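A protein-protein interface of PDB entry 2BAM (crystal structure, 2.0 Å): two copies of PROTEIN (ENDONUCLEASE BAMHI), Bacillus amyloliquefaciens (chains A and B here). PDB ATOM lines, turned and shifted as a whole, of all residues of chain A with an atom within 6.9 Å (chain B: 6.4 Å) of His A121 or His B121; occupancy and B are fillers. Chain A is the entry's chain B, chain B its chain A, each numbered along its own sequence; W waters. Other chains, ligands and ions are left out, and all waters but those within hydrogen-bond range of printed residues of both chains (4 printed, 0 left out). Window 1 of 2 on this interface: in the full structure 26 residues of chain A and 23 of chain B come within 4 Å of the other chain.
The side-chain amide nitrogen (ND2) of Asn A125 sits at hydrogen-bond distance from the side-chain amide oxygen (OD1) of Asn B125 (3.3 Å).
OG of Ser A118 lies within hydrogen-bond range of OG of Ser B118 (3.0 Å).
The side-chain amide nitrogen (ND2) of Asn A125 is in hydrogen-bond range of a ring nitrogen (ND1) of His B121, 3.4 Å away.
The backbone carbonyl oxygen (O) of Ser A119 sits at hydrogen-bond distance from the side-chain hydroxyl (OG) of Ser A123 (3.3 Å).
The side-chain amide oxygen of Asn B116 lies within hydrogen-bond range of the backbone NH of Ser B118, 2.9 Å away.
OD1 of Asn A116 is in hydrogen-bond range of OG of Ser A118, at 3.1 Å.
NH2 of Arg A122 lies within hydrogen-bond range of OG of Ser A119 (3.0 Å).
OG of Ser A119 lies within hydrogen-bond range of OE2 of Glu A113 (3.0 Å).
O of His A121 sits at hydrogen-bond distance from ND2 of Asn A125 (3.1 Å).
CB of Ser B118 touches CA of Ser A119, at 3.6 Å.
CA of Arg B122 touches CD2 of His A121 (3.5 Å).
Ile B117 touches Arg A122.
Arg A122 touches Ser B118.
CE of Met A124 touches OD1 of Asn B125, 3.7 Å away.
Asn A125 touches Tyr B165 (C to CE1, 3.9 Å).
Asn A125 touches Leu B168 (O to CD1, 3.5 Å).
CB of Asn B125 touches CD1 of Tyr A165, 3.9 Å away.
Tyr A165 touches Lys B126.
Leu A168 touches Asn B125 (CD1 to CB, 3.6 Å).
Glu A113 touches none of the printed residues of chain B.
Of the printed residues of chain B, Met A124 touches Asn B125 (3.7 Å).
Glu B113 touches none of the printed residues of chain A.
Of chain A, only His A121, Arg A122 and Asn A125 come within 4 Å of His B121.
Printed residues of chain A within 4 Å of Leu B168: Asn A125.
The nearest residue of chain B that does not touch His A121 is Ser B118 (4.8 Å).
The nearest residue of chain A that does not touch His B121 is Ser A118 (4.5 Å).
Of the 18 printed residues of chain B, 10 touch a printed residue of chain A.
Hydrophobic or aromatic side chains of chain B that line the printed part of chain A: Ile B117, His B121, Met B124, Tyr B165 and Leu B168.
Of the 18 printed residues of chain A, 10 touch a printed residue of chain B.
Hydrophobic or aromatic side chains of chain A within 4 Å of the printed part of chain B: Ile A117, His A121, Met A124, Tyr A165 and Leu A168.
Among the printed residues, no Asp or Glu carboxylate lies within 4 Å of a Lys or Arg side-chain nitrogen of the other chain.
Ile A117 touches Arg B122, and with the chains exchanged Arg A122 touches Ile B117.
Ser A118 touches its own counterpart, Ser B118.
Ser A118 touches Ser B119, and with the chains exchanged Ser A119 touches Ser B118.
Ser A118 touches Arg B122, and with the chains exchanged Arg A122 touches Ser B118.
17 positions are printed for both chains.
Of the 21 pairs that touch across the chains among the printed residues, 21 have their exchanged pair printed and touching as well.
Water W4 bridges the guanidinium group of Arg B122 (2.6 Å) and the side-chain amide oxygen of Asn A116 (2.7 Å).
Water W2 lies within hydrogen-bond range of the side-chain amide oxygen (OD1) of Asn B116 (2.6 Å) and the guanidinium group (NH1) of Arg A122 (2.8 Å).
Water W3 lies within hydrogen-bond range of OE1 of Glu A161 and NH1 of Arg B122.
Water W1 lies within hydrogen-bond range of OE1 of Glu B161 (2.9 Å) and NH1 of Arg A122 (2.9 Å).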
ATOM      1  N   GLU A 113     -18.700  19.669   2.411  1.00  0.00           N
ATOM      2  CA  GLU A 113     -17.821  18.781   3.140  1.00  0.00           C
ATOM      3  C   GLU A 113     -18.352  17.423   3.543  1.00  0.00           C
ATOM      4  O   GLU A 113     -19.154  17.310   4.470  1.00  0.00           O
ATOM      5  CB  GLU A 113     -17.283  19.473   4.395  1.00  0.00           C
ATOM      6  CG  GLU A 113     -15.872  20.012   4.278  1.00  0.00           C
ATOM      7  CD  GLU A 113     -14.851  18.960   3.914  1.00  0.00           C
ATOM      8  OE1 GLU A 113     -15.048  17.769   4.208  1.00  0.00           O
ATOM      9  OE2 GLU A 113     -13.824  19.335   3.335  1.00  0.00           O
ATOM     10  N   ASN A 116     -13.273  13.861   5.820  1.00  0.00           N
ATOM     11  CA  ASN A 116     -13.036  13.642   7.231  1.00  0.00           C
ATOM     12  C   ASN A 116     -13.278  14.975   7.918  1.00  0.00           C
ATOM     13  O   ASN A 116     -13.086  16.021   7.309  1.00  0.00           O
ATOM     14  CB  ASN A 116     -11.594  13.188   7.409  1.00  0.00           C
ATOM     15  CG  ASN A 116     -11.339  12.565   8.762  1.00  0.00           C
ATOM     16  OD1 ASN A 116     -11.127  13.278   9.748  1.00  0.00           O
ATOM     17  ND2 ASN A 116     -11.293  11.222   8.805  1.00  0.00           N
ATOM     18  N   ILE A 117     -13.738  14.934   9.172  1.00  0.00           N
ATOM     19  CA  ILE A 117     -13.999  16.159   9.949  1.00  0.00           C
ATOM     20  C   ILE A 117     -12.783  17.112   9.960  1.00  0.00           C
ATOM     21  O   ILE A 117     -12.942  18.327   9.948  1.00  0.00           O
ATOM     22  CB  ILE A 117     -14.489  15.833  11.397  1.00  0.00           C
ATOM     23  CG1 ILE A 117     -14.577  17.092  12.254  1.00  0.00           C
ATOM     24  CG2 ILE A 117     -13.579  14.822  12.064  1.00  0.00           C
ATOM     25  CD1 ILE A 117     -15.726  18.005  11.893  1.00  0.00           C
ATOM     26  N   SER A 118     -11.570  16.561   9.956  1.00  0.00           N
ATOM     27  CA  SER A 118     -10.356  17.375   9.937  1.00  0.00           C
ATOM     28  C   SER A 118     -10.274  18.185   8.641  1.00  0.00           C
ATOM     29  O   SER A 118      -9.803  19.327   8.645  1.00  0.00           O
ATOM     30  CB  SER A 118      -9.115  16.493  10.102  1.00  0.00           C
ATOM     31  OG  SER A 118      -9.020  15.503   9.080  1.00  0.00           O
ATOM     32  N   SER A 119     -10.783  17.610   7.558  1.00  0.00           N
ATOM     33  CA  SER A 119     -10.815  18.260   6.239  1.00  0.00           C
ATOM     34  C   SER A 119     -11.734  19.484   6.282  1.00  0.00           C
ATOM     35  O   SER A 119     -11.537  20.440   5.525  1.00  0.00           O
ATOM     36  CB  SER A 119     -11.311  17.262   5.163  1.00  0.00           C
ATOM     37  OG  SER A 119     -11.264  17.773   3.850  1.00  0.00           O
ATOM     38  N   ALA A 120     -12.746  19.444   7.161  1.00  0.00           N
ATOM     39  CA  ALA A 120     -13.701  20.539   7.305  1.00  0.00           C
ATOM     40  C   ALA A 120     -12.999  21.765   7.865  1.00  0.00           C
ATOM     41  O   ALA A 120     -13.385  22.889   7.554  1.00  0.00           O
ATOM     42  CB  ALA A 120     -14.845  20.123   8.193  1.00  0.00           C
ATOM     43  N   HIS A 121     -11.965  21.555   8.689  1.00  0.00           N
ATOM     44  CA  HIS A 121     -11.218  22.679   9.246  1.00  0.00           C
ATOM     45  C   HIS A 121     -10.423  23.333   8.117  1.00  0.00           C
ATOM     46  O   HIS A 121     -10.205  24.541   8.127  1.00  0.00           O
ATOM     47  CB  HIS A 121     -10.286  22.244  10.372  1.00  0.00           C
ATOM     48  CG  HIS A 121     -10.986  21.873  11.635  1.00  0.00           C
ATOM     49  ND1 HIS A 121     -11.651  20.668  11.798  1.00  0.00           N
ATOM     50  CD2 HIS A 121     -11.062  22.493  12.838  1.00  0.00           C
ATOM     51  CE1 HIS A 121     -12.093  20.569  13.030  1.00  0.00           C
ATOM     52  NE2 HIS A 121     -11.744  21.666  13.687  1.00  0.00           N
ATOM     53  N   ARG A 122      -9.997  22.530   7.148  1.00  0.00           N
ATOM     54  CA  ARG A 122      -9.278  23.064   6.004  1.00  0.00           C
ATOM     55  C   ARG A 122     -10.249  23.897   5.181  1.00  0.00           C
ATOM     56  O   ARG A 122      -9.956  25.036   4.838  1.00  0.00           O
ATOM     57  CB  ARG A 122      -8.662  21.933   5.172  1.00  0.00           C
ATOM     58  CG  ARG A 122      -7.967  22.394   3.905  1.00  0.00           C
ATOM     59  CD  ARG A 122      -7.199  21.263   3.217  1.00  0.00           C
ATOM     60  NE  ARG A 122      -8.051  20.098   2.976  1.00  0.00           N
ATOM     61  CZ  ARG A 122      -7.615  18.856   2.816  1.00  0.00           C
ATOM     62  NH1 ARG A 122      -6.315  18.591   2.848  1.00  0.00           N
ATOM     63  NH2 ARG A 122      -8.473  17.851   2.682  1.00  0.00           N
ATOM     64  N   SER A 123     -11.426  23.337   4.926  1.00  0.00           N
ATOM     65  CA  SER A 123     -12.470  24.019   4.160  1.00  0.00           C
ATOM     66  C   SER A 123     -12.793  25.380   4.749  1.00  0.00           C
ATOM     67  O   SER A 123     -12.795  26.376   4.048  1.00  0.00           O
ATOM     68  CB  SER A 123     -13.751  23.186   4.110  1.00  0.00           C
ATOM     69  OG  SER A 123     -13.547  22.003   3.371  1.00  0.00           O
ATOM     70  N   MET A 124     -13.056  25.411   6.051  1.00  0.00           N
ATOM     71  CA  MET A 124     -13.377  26.653   6.743  1.00  0.00           C
ATOM     72  C   MET A 124     -12.223  27.655   6.703  1.00  0.00           C
ATOM     73  O   MET A 124     -12.430  28.844   6.463  1.00  0.00           O
ATOM     74  CB  MET A 124     -13.807  26.364   8.187  1.00  0.00           C
ATOM     75  CG  MET A 124     -14.096  27.620   9.023  1.00  0.00           C
ATOM     76  SD  MET A 124     -14.526  27.245  10.730  1.00  0.00           S
ATOM     77  CE  MET A 124     -12.895  26.770  11.395  1.00  0.00           C
ATOM     78  N   ASN A 125     -11.005  27.167   6.930  1.00  0.00           N
ATOM     79  CA  ASN A 125      -9.825  28.026   6.883  1.00  0.00           C
ATOM     80  C   ASN A 125      -9.567  28.584   5.480  1.00  0.00           C
ATOM     81  O   ASN A 125      -9.063  29.699   5.343  1.00  0.00           O
ATOM     82  CB  ASN A 125      -8.591  27.284   7.379  1.00  0.00           C
ATOM     83  CG  ASN A 125      -8.567  27.145   8.890  1.00  0.00           C
ATOM     84  OD1 ASN A 125      -9.177  27.938   9.611  1.00  0.00           O
ATOM     85  ND2 ASN A 125      -7.839  26.146   9.376  1.00  0.00           N
ATOM     86  N   LYS A 126      -9.880  27.803   4.455  1.00  0.00           N
ATOM     87  CA  LYS A 126      -9.708  28.242   3.077  1.00  0.00           C
ATOM     88  C   LYS A 126     -10.750  29.318   2.723  1.00  0.00           C
ATOM     89  O   LYS A 126     -10.437  30.301   2.036  1.00  0.00           O
ATOM     90  CB  LYS A 126      -9.799  27.033   2.128  1.00  0.00           C
ATOM     91  CG  LYS A 126      -9.454  27.332   0.650  1.00  0.00           C
ATOM     92  CD  LYS A 126      -9.841  26.205  -0.299  1.00  0.00           C
ATOM     93  CE  LYS A 126      -8.749  25.142  -0.353  1.00  0.00           C
ATOM     94  NZ  LYS A 126      -9.262  23.900  -1.039  1.00  0.00           N
ATOM     95  N   ILE A 141     -20.665  26.323   4.208  1.00  0.00           N
ATOM     96  CA  ILE A 141     -20.193  24.966   4.368  1.00  0.00           C
ATOM     97  C   ILE A 141     -21.404  24.048   4.573  1.00  0.00           C
ATOM     98  O   ILE A 141     -22.255  24.305   5.429  1.00  0.00           O
ATOM     99  CB  ILE A 141     -19.204  24.854   5.544  1.00  0.00           C
ATOM    100  CG1 ILE A 141     -17.857  25.458   5.139  1.00  0.00           C
ATOM    101  CG2 ILE A 141     -19.021  23.395   5.959  1.00  0.00           C
ATOM    102  CD1 ILE A 141     -16.798  25.409   6.202  1.00  0.00           C
ATOM    103  N   THR A 157     -17.221  14.551   8.101  1.00  0.00           N
ATOM    104  CA  THR A 157     -17.524  15.863   8.650  1.00  0.00           C
ATOM    105  C   THR A 157     -18.979  15.823   9.114  1.00  0.00           C
ATOM    106  O   THR A 157     -19.808  15.147   8.488  1.00  0.00           O
ATOM    107  CB  THR A 157     -17.375  16.948   7.574  1.00  0.00           C
ATOM    108  OG1 THR A 157     -16.027  16.948   7.109  1.00  0.00           O
ATOM    109  CG2 THR A 157     -17.719  18.312   8.117  1.00  0.00           C
ATOM    110  N   GLU A 161     -19.648  18.289  15.277  1.00  0.00           N
ATOM    111  CA  GLU A 161     -18.218  18.206  15.520  1.00  0.00           C
ATOM    112  C   GLU A 161     -17.412  19.420  15.047  1.00  0.00           C
ATOM    113  O   GLU A 161     -16.327  19.678  15.554  1.00  0.00           O
ATOM    114  CB  GLU A 161     -17.644  16.913  14.954  1.00  0.00           C
ATOM    115  CG  GLU A 161     -16.238  16.670  15.423  1.00  0.00           C
ATOM    116  CD  GLU A 161     -15.773  15.224  15.292  1.00  0.00           C
ATOM    117  OE1 GLU A 161     -14.764  14.877  15.952  1.00  0.00           O
ATOM    118  OE2 GLU A 161     -16.406  14.456  14.537  1.00  0.00           O
ATOM    119  N   LEU A 162     -17.922  20.162  14.072  1.00  0.00           N
ATOM    120  CA  LEU A 162     -17.215  21.349  13.608  1.00  0.00           C
ATOM    121  C   LEU A 162     -17.684  22.530  14.443  1.00  0.00           C
ATOM    122  O   LEU A 162     -16.970  23.499  14.609  1.00  0.00           O
ATOM    123  CB  LEU A 162     -17.490  21.624  12.118  1.00  0.00           C
ATOM    124  CG  LEU A 162     -16.507  22.611  11.453  1.00  0.00           C
ATOM    125  CD1 LEU A 162     -15.103  22.053  11.526  1.00  0.00           C
ATOM    126  CD2 LEU A 162     -16.890  22.876  10.016  1.00  0.00           C
ATOM    127  N   TYR A 165     -15.796  25.045  16.642  1.00  0.00           N
ATOM    128  CA  TYR A 165     -14.940  25.937  15.888  1.00  0.00           C
ATOM    129  C   TYR A 165     -15.610  27.012  15.022  1.00  0.00           C
ATOM    130  O   TYR A 165     -14.931  27.755  14.327  1.00  0.00           O
ATOM    131  CB  TYR A 165     -13.966  25.094  15.069  1.00  0.00           C
ATOM    132  CG  TYR A 165     -13.192  24.096  15.903  1.00  0.00           C
ATOM    133  CD1 TYR A 165     -12.019  24.466  16.542  1.00  0.00           C
ATOM    134  CD2 TYR A 165     -13.627  22.783  16.039  1.00  0.00           C
ATOM    135  CE1 TYR A 165     -11.277  23.553  17.303  1.00  0.00           C
ATOM    136  CE2 TYR A 165     -12.895  21.852  16.791  1.00  0.00           C
ATOM    137  CZ  TYR A 165     -11.713  22.246  17.423  1.00  0.00           C
ATOM    138  OH  TYR A 165     -10.963  21.344  18.140  1.00  0.00           O
ATOM    139  N   LEU A 168     -14.463  30.729  15.240  1.00  0.00           N
ATOM    140  CA  LEU A 168     -13.250  31.202  14.589  1.00  0.00           C
ATOM    141  C   LEU A 168     -13.563  31.970  13.298  1.00  0.00           C
ATOM    142  O   LEU A 168     -12.685  32.551  12.684  1.00  0.00           O
ATOM    143  CB  LEU A 168     -12.291  30.035  14.321  1.00  0.00           C
ATOM    144  CG  LEU A 168     -11.687  29.414  15.571  1.00  0.00           C
ATOM    145  CD1 LEU A 168     -10.880  28.192  15.219  1.00  0.00           C
ATOM    146  CD2 LEU A 168     -10.826  30.429  16.285  1.00  0.00           C
ATOM    147  N   GLU B 113       2.362  17.045  14.767  1.00  0.00           N
ATOM    148  CA  GLU B 113       1.572  16.485  13.683  1.00  0.00           C
ATOM    149  C   GLU B 113       2.183  15.537  12.669  1.00  0.00           C
ATOM    150  O   GLU B 113       3.071  15.889  11.921  1.00  0.00           O
ATOM    151  CB  GLU B 113       0.852  17.602  12.924  1.00  0.00           C
ATOM    152  CG  GLU B 113      -0.498  18.047  13.508  1.00  0.00           C
ATOM    153  CD  GLU B 113      -1.637  17.066  13.251  1.00  0.00           C
ATOM    154  OE1 GLU B 113      -2.763  17.377  13.656  1.00  0.00           O
ATOM    155  OE2 GLU B 113      -1.432  15.972  12.674  1.00  0.00           O
ATOM    156  N   ASN B 116      -2.943  13.270   8.937  1.00  0.00           N
ATOM    157  CA  ASN B 116      -3.220  13.872   7.638  1.00  0.00           C
ATOM    158  C   ASN B 116      -3.047  15.390   7.704  1.00  0.00           C
ATOM    159  O   ASN B 116      -3.258  16.003   8.748  1.00  0.00           O
ATOM    160  CB  ASN B 116      -4.650  13.529   7.202  1.00  0.00           C
ATOM    161  CG  ASN B 116      -4.912  13.869   5.756  1.00  0.00           C
ATOM    162  OD1 ASN B 116      -4.944  15.042   5.369  1.00  0.00           O
ATOM    163  ND2 ASN B 116      -5.127  12.836   4.950  1.00  0.00           N
ATOM    164  N   ILE B 117      -2.639  16.004   6.593  1.00  0.00           N
ATOM    165  CA  ILE B 117      -2.455  17.449   6.553  1.00  0.00           C
ATOM    166  C   ILE B 117      -3.743  18.163   7.009  1.00  0.00           C
ATOM    167  O   ILE B 117      -3.667  19.248   7.612  1.00  0.00           O
ATOM    168  CB  ILE B 117      -2.011  17.931   5.128  1.00  0.00           C
ATOM    169  CG1 ILE B 117      -1.987  19.470   5.051  1.00  0.00           C
ATOM    170  CG2 ILE B 117      -2.948  17.402   4.049  1.00  0.00           C
ATOM    171  CD1 ILE B 117      -0.976  20.134   5.997  1.00  0.00           C
ATOM    172  N   SER B 118      -4.902  17.564   6.749  1.00  0.00           N
ATOM    173  CA  SER B 118      -6.144  18.189   7.170  1.00  0.00           C
ATOM    174  C   SER B 118      -6.269  18.167   8.690  1.00  0.00           C
ATOM    175  O   SER B 118      -6.903  19.032   9.270  1.00  0.00           O
ATOM    176  CB  SER B 118      -7.346  17.529   6.495  1.00  0.00           C
ATOM    177  OG  SER B 118      -7.378  16.128   6.699  1.00  0.00           O
ATOM    178  N   SER B 119      -5.650  17.178   9.326  1.00  0.00           N
ATOM    179  CA  SER B 119      -5.665  17.067  10.776  1.00  0.00           C
ATOM    180  C   SER B 119      -4.902  18.238  11.395  1.00  0.00           C
ATOM    181  O   SER B 119      -5.234  18.677  12.498  1.00  0.00           O
ATOM    182  CB  SER B 119      -5.051  15.748  11.236  1.00  0.00           C
ATOM    183  OG  SER B 119      -4.911  15.712  12.639  1.00  0.00           O
ATOM    184  N   ALA B 120      -3.892  18.762  10.688  1.00  0.00           N
ATOM    185  CA  ALA B 120      -3.111  19.891  11.190  1.00  0.00           C
ATOM    186  C   ALA B 120      -3.934  21.173  11.250  1.00  0.00           C
ATOM    187  O   ALA B 120      -3.666  22.041  12.076  1.00  0.00           O
ATOM    188  CB  ALA B 120      -1.875  20.103  10.350  1.00  0.00           C
ATOM    189  N   HIS B 121      -4.931  21.311  10.376  1.00  0.00           N
ATOM    190  CA  HIS B 121      -5.783  22.496  10.398  1.00  0.00           C
ATOM    191  C   HIS B 121      -6.594  22.485  11.686  1.00  0.00           C
ATOM    192  O   HIS B 121      -6.756  23.527  12.320  1.00  0.00           O
ATOM    193  CB  HIS B 121      -6.709  22.525   9.189  1.00  0.00           C
ATOM    194  CG  HIS B 121      -6.003  22.816   7.911  1.00  0.00           C
ATOM    195  ND1 HIS B 121      -5.894  24.098   7.395  1.00  0.00           N
ATOM    196  CD2 HIS B 121      -5.350  22.011   7.050  1.00  0.00           C
ATOM    197  CE1 HIS B 121      -5.206  24.053   6.279  1.00  0.00           C
ATOM    198  NE2 HIS B 121      -4.860  22.798   6.040  1.00  0.00           N
ATOM    199  N   ARG B 122      -7.081  21.309  12.073  1.00  0.00           N
ATOM    200  CA  ARG B 122      -7.838  21.145  13.317  1.00  0.00           C
ATOM    201  C   ARG B 122      -6.938  21.530  14.504  1.00  0.00           C
ATOM    202  O   ARG B 122      -7.348  22.293  15.400  1.00  0.00           O
ATOM    203  CB  ARG B 122      -8.298  19.686  13.472  1.00  0.00           C
ATOM    204  CG  ARG B 122      -9.017  19.384  14.797  1.00  0.00           C
ATOM    205  CD  ARG B 122      -9.564  17.991  14.842  1.00  0.00           C
ATOM    206  NE  ARG B 122      -8.532  17.003  14.552  1.00  0.00           N
ATOM    207  CZ  ARG B 122      -8.755  15.832  13.957  1.00  0.00           C
ATOM    208  NH1 ARG B 122      -9.990  15.512  13.602  1.00  0.00           N
ATOM    209  NH2 ARG B 122      -7.742  15.008  13.679  1.00  0.00           N
ATOM    210  N   SER B 123      -5.705  21.017  14.477  1.00  0.00           N
ATOM    211  CA  SER B 123      -4.707  21.285  15.506  1.00  0.00           C
ATOM    212  C   SER B 123      -4.439  22.763  15.667  1.00  0.00           C
ATOM    213  O   SER B 123      -4.300  23.249  16.787  1.00  0.00           O
ATOM    214  CB  SER B 123      -3.411  20.592  15.150  1.00  0.00           C
ATOM    215  OG  SER B 123      -3.617  19.201  15.095  1.00  0.00           O
ATOM    216  N   MET B 124      -4.321  23.466  14.535  1.00  0.00           N
ATOM    217  CA  MET B 124      -4.085  24.897  14.542  1.00  0.00           C
ATOM    218  C   MET B 124      -5.287  25.639  15.113  1.00  0.00           C
ATOM    219  O   MET B 124      -5.122  26.574  15.898  1.00  0.00           O
ATOM    220  CB  MET B 124      -3.797  25.402  13.128  1.00  0.00           C
ATOM    221  CG  MET B 124      -3.607  26.914  13.017  1.00  0.00           C
ATOM    222  SD  MET B 124      -3.034  27.477  11.433  1.00  0.00           S
ATOM    223  CE  MET B 124      -4.334  26.899  10.329  1.00  0.00           C
ATOM    224  N   ASN B 125      -6.483  25.202  14.730  1.00  0.00           N
ATOM    225  CA  ASN B 125      -7.722  25.819  15.177  1.00  0.00           C
ATOM    226  C   ASN B 125      -7.967  25.598  16.657  1.00  0.00           C
ATOM    227  O   ASN B 125      -8.475  26.496  17.350  1.00  0.00           O
ATOM    228  CB  ASN B 125      -8.913  25.322  14.340  1.00  0.00           C
ATOM    229  CG  ASN B 125      -8.870  25.811  12.896  1.00  0.00           C
ATOM    230  OD1 ASN B 125      -9.531  25.257  12.039  1.00  0.00           O
ATOM    231  ND2 ASN B 125      -8.089  26.853  12.631  1.00  0.00           N
ATOM    232  N   LYS B 126      -7.614  24.411  17.143  1.00  0.00           N
ATOM    233  CA  LYS B 126      -7.796  24.107  18.562  1.00  0.00           C
ATOM    234  C   LYS B 126      -6.904  25.005  19.413  1.00  0.00           C
ATOM    235  O   LYS B 126      -7.338  25.547  20.421  1.00  0.00           O
ATOM    236  CB  LYS B 126      -7.491  22.638  18.843  1.00  0.00           C
ATOM    237  CG  LYS B 126      -7.707  22.226  20.267  1.00  0.00           C
ATOM    238  CD  LYS B 126      -7.521  20.733  20.456  1.00  0.00           C
ATOM    239  CE  LYS B 126      -8.586  19.928  19.737  1.00  0.00           C
ATOM    240  NZ  LYS B 126      -8.325  18.468  19.838  1.00  0.00           N
ATOM    241  N   LEU B 128      -5.702  27.865  18.393  1.00  0.00           N
ATOM    242  CA  LEU B 128      -6.169  29.234  18.190  1.00  0.00           C
ATOM    243  C   LEU B 128      -7.313  29.494  19.163  1.00  0.00           C
ATOM    244  O   LEU B 128      -7.423  30.568  19.740  1.00  0.00           O
ATOM    245  CB  LEU B 128      -6.661  29.438  16.751  1.00  0.00           C
ATOM    246  CG  LEU B 128      -5.586  29.470  15.669  1.00  0.00           C
ATOM    247  CD1 LEU B 128      -6.225  29.515  14.295  1.00  0.00           C
ATOM    248  CD2 LEU B 128      -4.666  30.667  15.911  1.00  0.00           C
ATOM    249  N   THR B 157       0.917  15.465   7.442  1.00  0.00           N
ATOM    250  CA  THR B 157       1.250  16.868   7.642  1.00  0.00           C
ATOM    251  C   THR B 157       2.664  17.242   7.256  1.00  0.00           C
ATOM    252  O   THR B 157       3.617  16.640   7.715  1.00  0.00           O
ATOM    253  CB  THR B 157       1.005  17.312   9.086  1.00  0.00           C
ATOM    254  OG1 THR B 157      -0.377  17.108   9.414  1.00  0.00           O
ATOM    255  CG2 THR B 157       1.340  18.774   9.255  1.00  0.00           C
ATOM    256  N   GLU B 161       2.751  22.587   3.059  1.00  0.00           N
ATOM    257  CA  GLU B 161       1.320  22.538   2.746  1.00  0.00           C
ATOM    258  C   GLU B 161       0.438  23.319   3.748  1.00  0.00           C
ATOM    259  O   GLU B 161      -0.574  23.901   3.369  1.00  0.00           O
ATOM    260  CB  GLU B 161       0.854  21.089   2.614  1.00  0.00           C
ATOM    261  CG  GLU B 161      -0.559  20.951   2.067  1.00  0.00           C
ATOM    262  CD  GLU B 161      -0.840  19.617   1.378  1.00  0.00           C
ATOM    263  OE1 GLU B 161      -1.903  19.530   0.740  1.00  0.00           O
ATOM    264  OE2 GLU B 161      -0.006  18.685   1.436  1.00  0.00           O
ATOM    265  N   LEU B 162       0.828  23.356   5.019  1.00  0.00           N
ATOM    266  CA  LEU B 162       0.071  24.117   6.008  1.00  0.00           C
ATOM    267  C   LEU B 162       0.496  25.590   5.963  1.00  0.00           C
ATOM    268  O   LEU B 162      -0.263  26.463   6.389  1.00  0.00           O
ATOM    269  CB  LEU B 162       0.274  23.559   7.429  1.00  0.00           C
ATOM    270  CG  LEU B 162      -0.572  24.240   8.518  1.00  0.00           C
ATOM    271  CD1 LEU B 162      -2.030  23.995   8.226  1.00  0.00           C
ATOM    272  CD2 LEU B 162      -0.228  23.754   9.905  1.00  0.00           C
ATOM    273  N   TYR B 165      -1.543  28.814   5.310  1.00  0.00           N
ATOM    274  CA  TYR B 165      -2.534  29.104   6.318  1.00  0.00           C
ATOM    275  C   TYR B 165      -1.965  29.698   7.593  1.00  0.00           C
ATOM    276  O   TYR B 165      -2.708  30.098   8.464  1.00  0.00           O
ATOM    277  CB  TYR B 165      -3.309  27.827   6.618  1.00  0.00           C
ATOM    278  CG  TYR B 165      -4.103  27.333   5.441  1.00  0.00           C
ATOM    279  CD1 TYR B 165      -5.366  27.848   5.172  1.00  0.00           C
ATOM    280  CD2 TYR B 165      -3.603  26.356   4.603  1.00  0.00           C
ATOM    281  CE1 TYR B 165      -6.107  27.399   4.101  1.00  0.00           C
ATOM    282  CE2 TYR B 165      -4.339  25.900   3.518  1.00  0.00           C
ATOM    283  CZ  TYR B 165      -5.587  26.428   3.280  1.00  0.00           C
ATOM    284  OH  TYR B 165      -6.336  25.993   2.219  1.00  0.00           O
ATOM    285  N   LEU B 168      -3.413  32.902   9.245  1.00  0.00           N
ATOM    286  CA  LEU B 168      -4.659  32.860   9.989  1.00  0.00           C
ATOM    287  C   LEU B 168      -4.399  32.912  11.500  1.00  0.00           C
ATOM    288  O   LEU B 168      -5.330  32.836  12.303  1.00  0.00           O
ATOM    289  CB  LEU B 168      -5.447  31.603   9.622  1.00  0.00           C
ATOM    290  CG  LEU B 168      -6.004  31.612   8.198  1.00  0.00           C
ATOM    291  CD1 LEU B 168      -6.715  30.312   7.894  1.00  0.00           C
ATOM    292  CD2 LEU B 168      -6.945  32.795   8.024  1.00  0.00           C
HETATM  293  O   HOH W   1      -4.343  20.486   1.915  1.00  0.00           O
HETATM  294  O   HOH W   2      -6.163  15.835   3.216  1.00  0.00           O
HETATM  295  O   HOH W   3     -12.430  16.329  15.287  1.00  0.00           O
HETATM  296  O   HOH W   4     -10.127  13.339  12.271  1.00  0.00           O
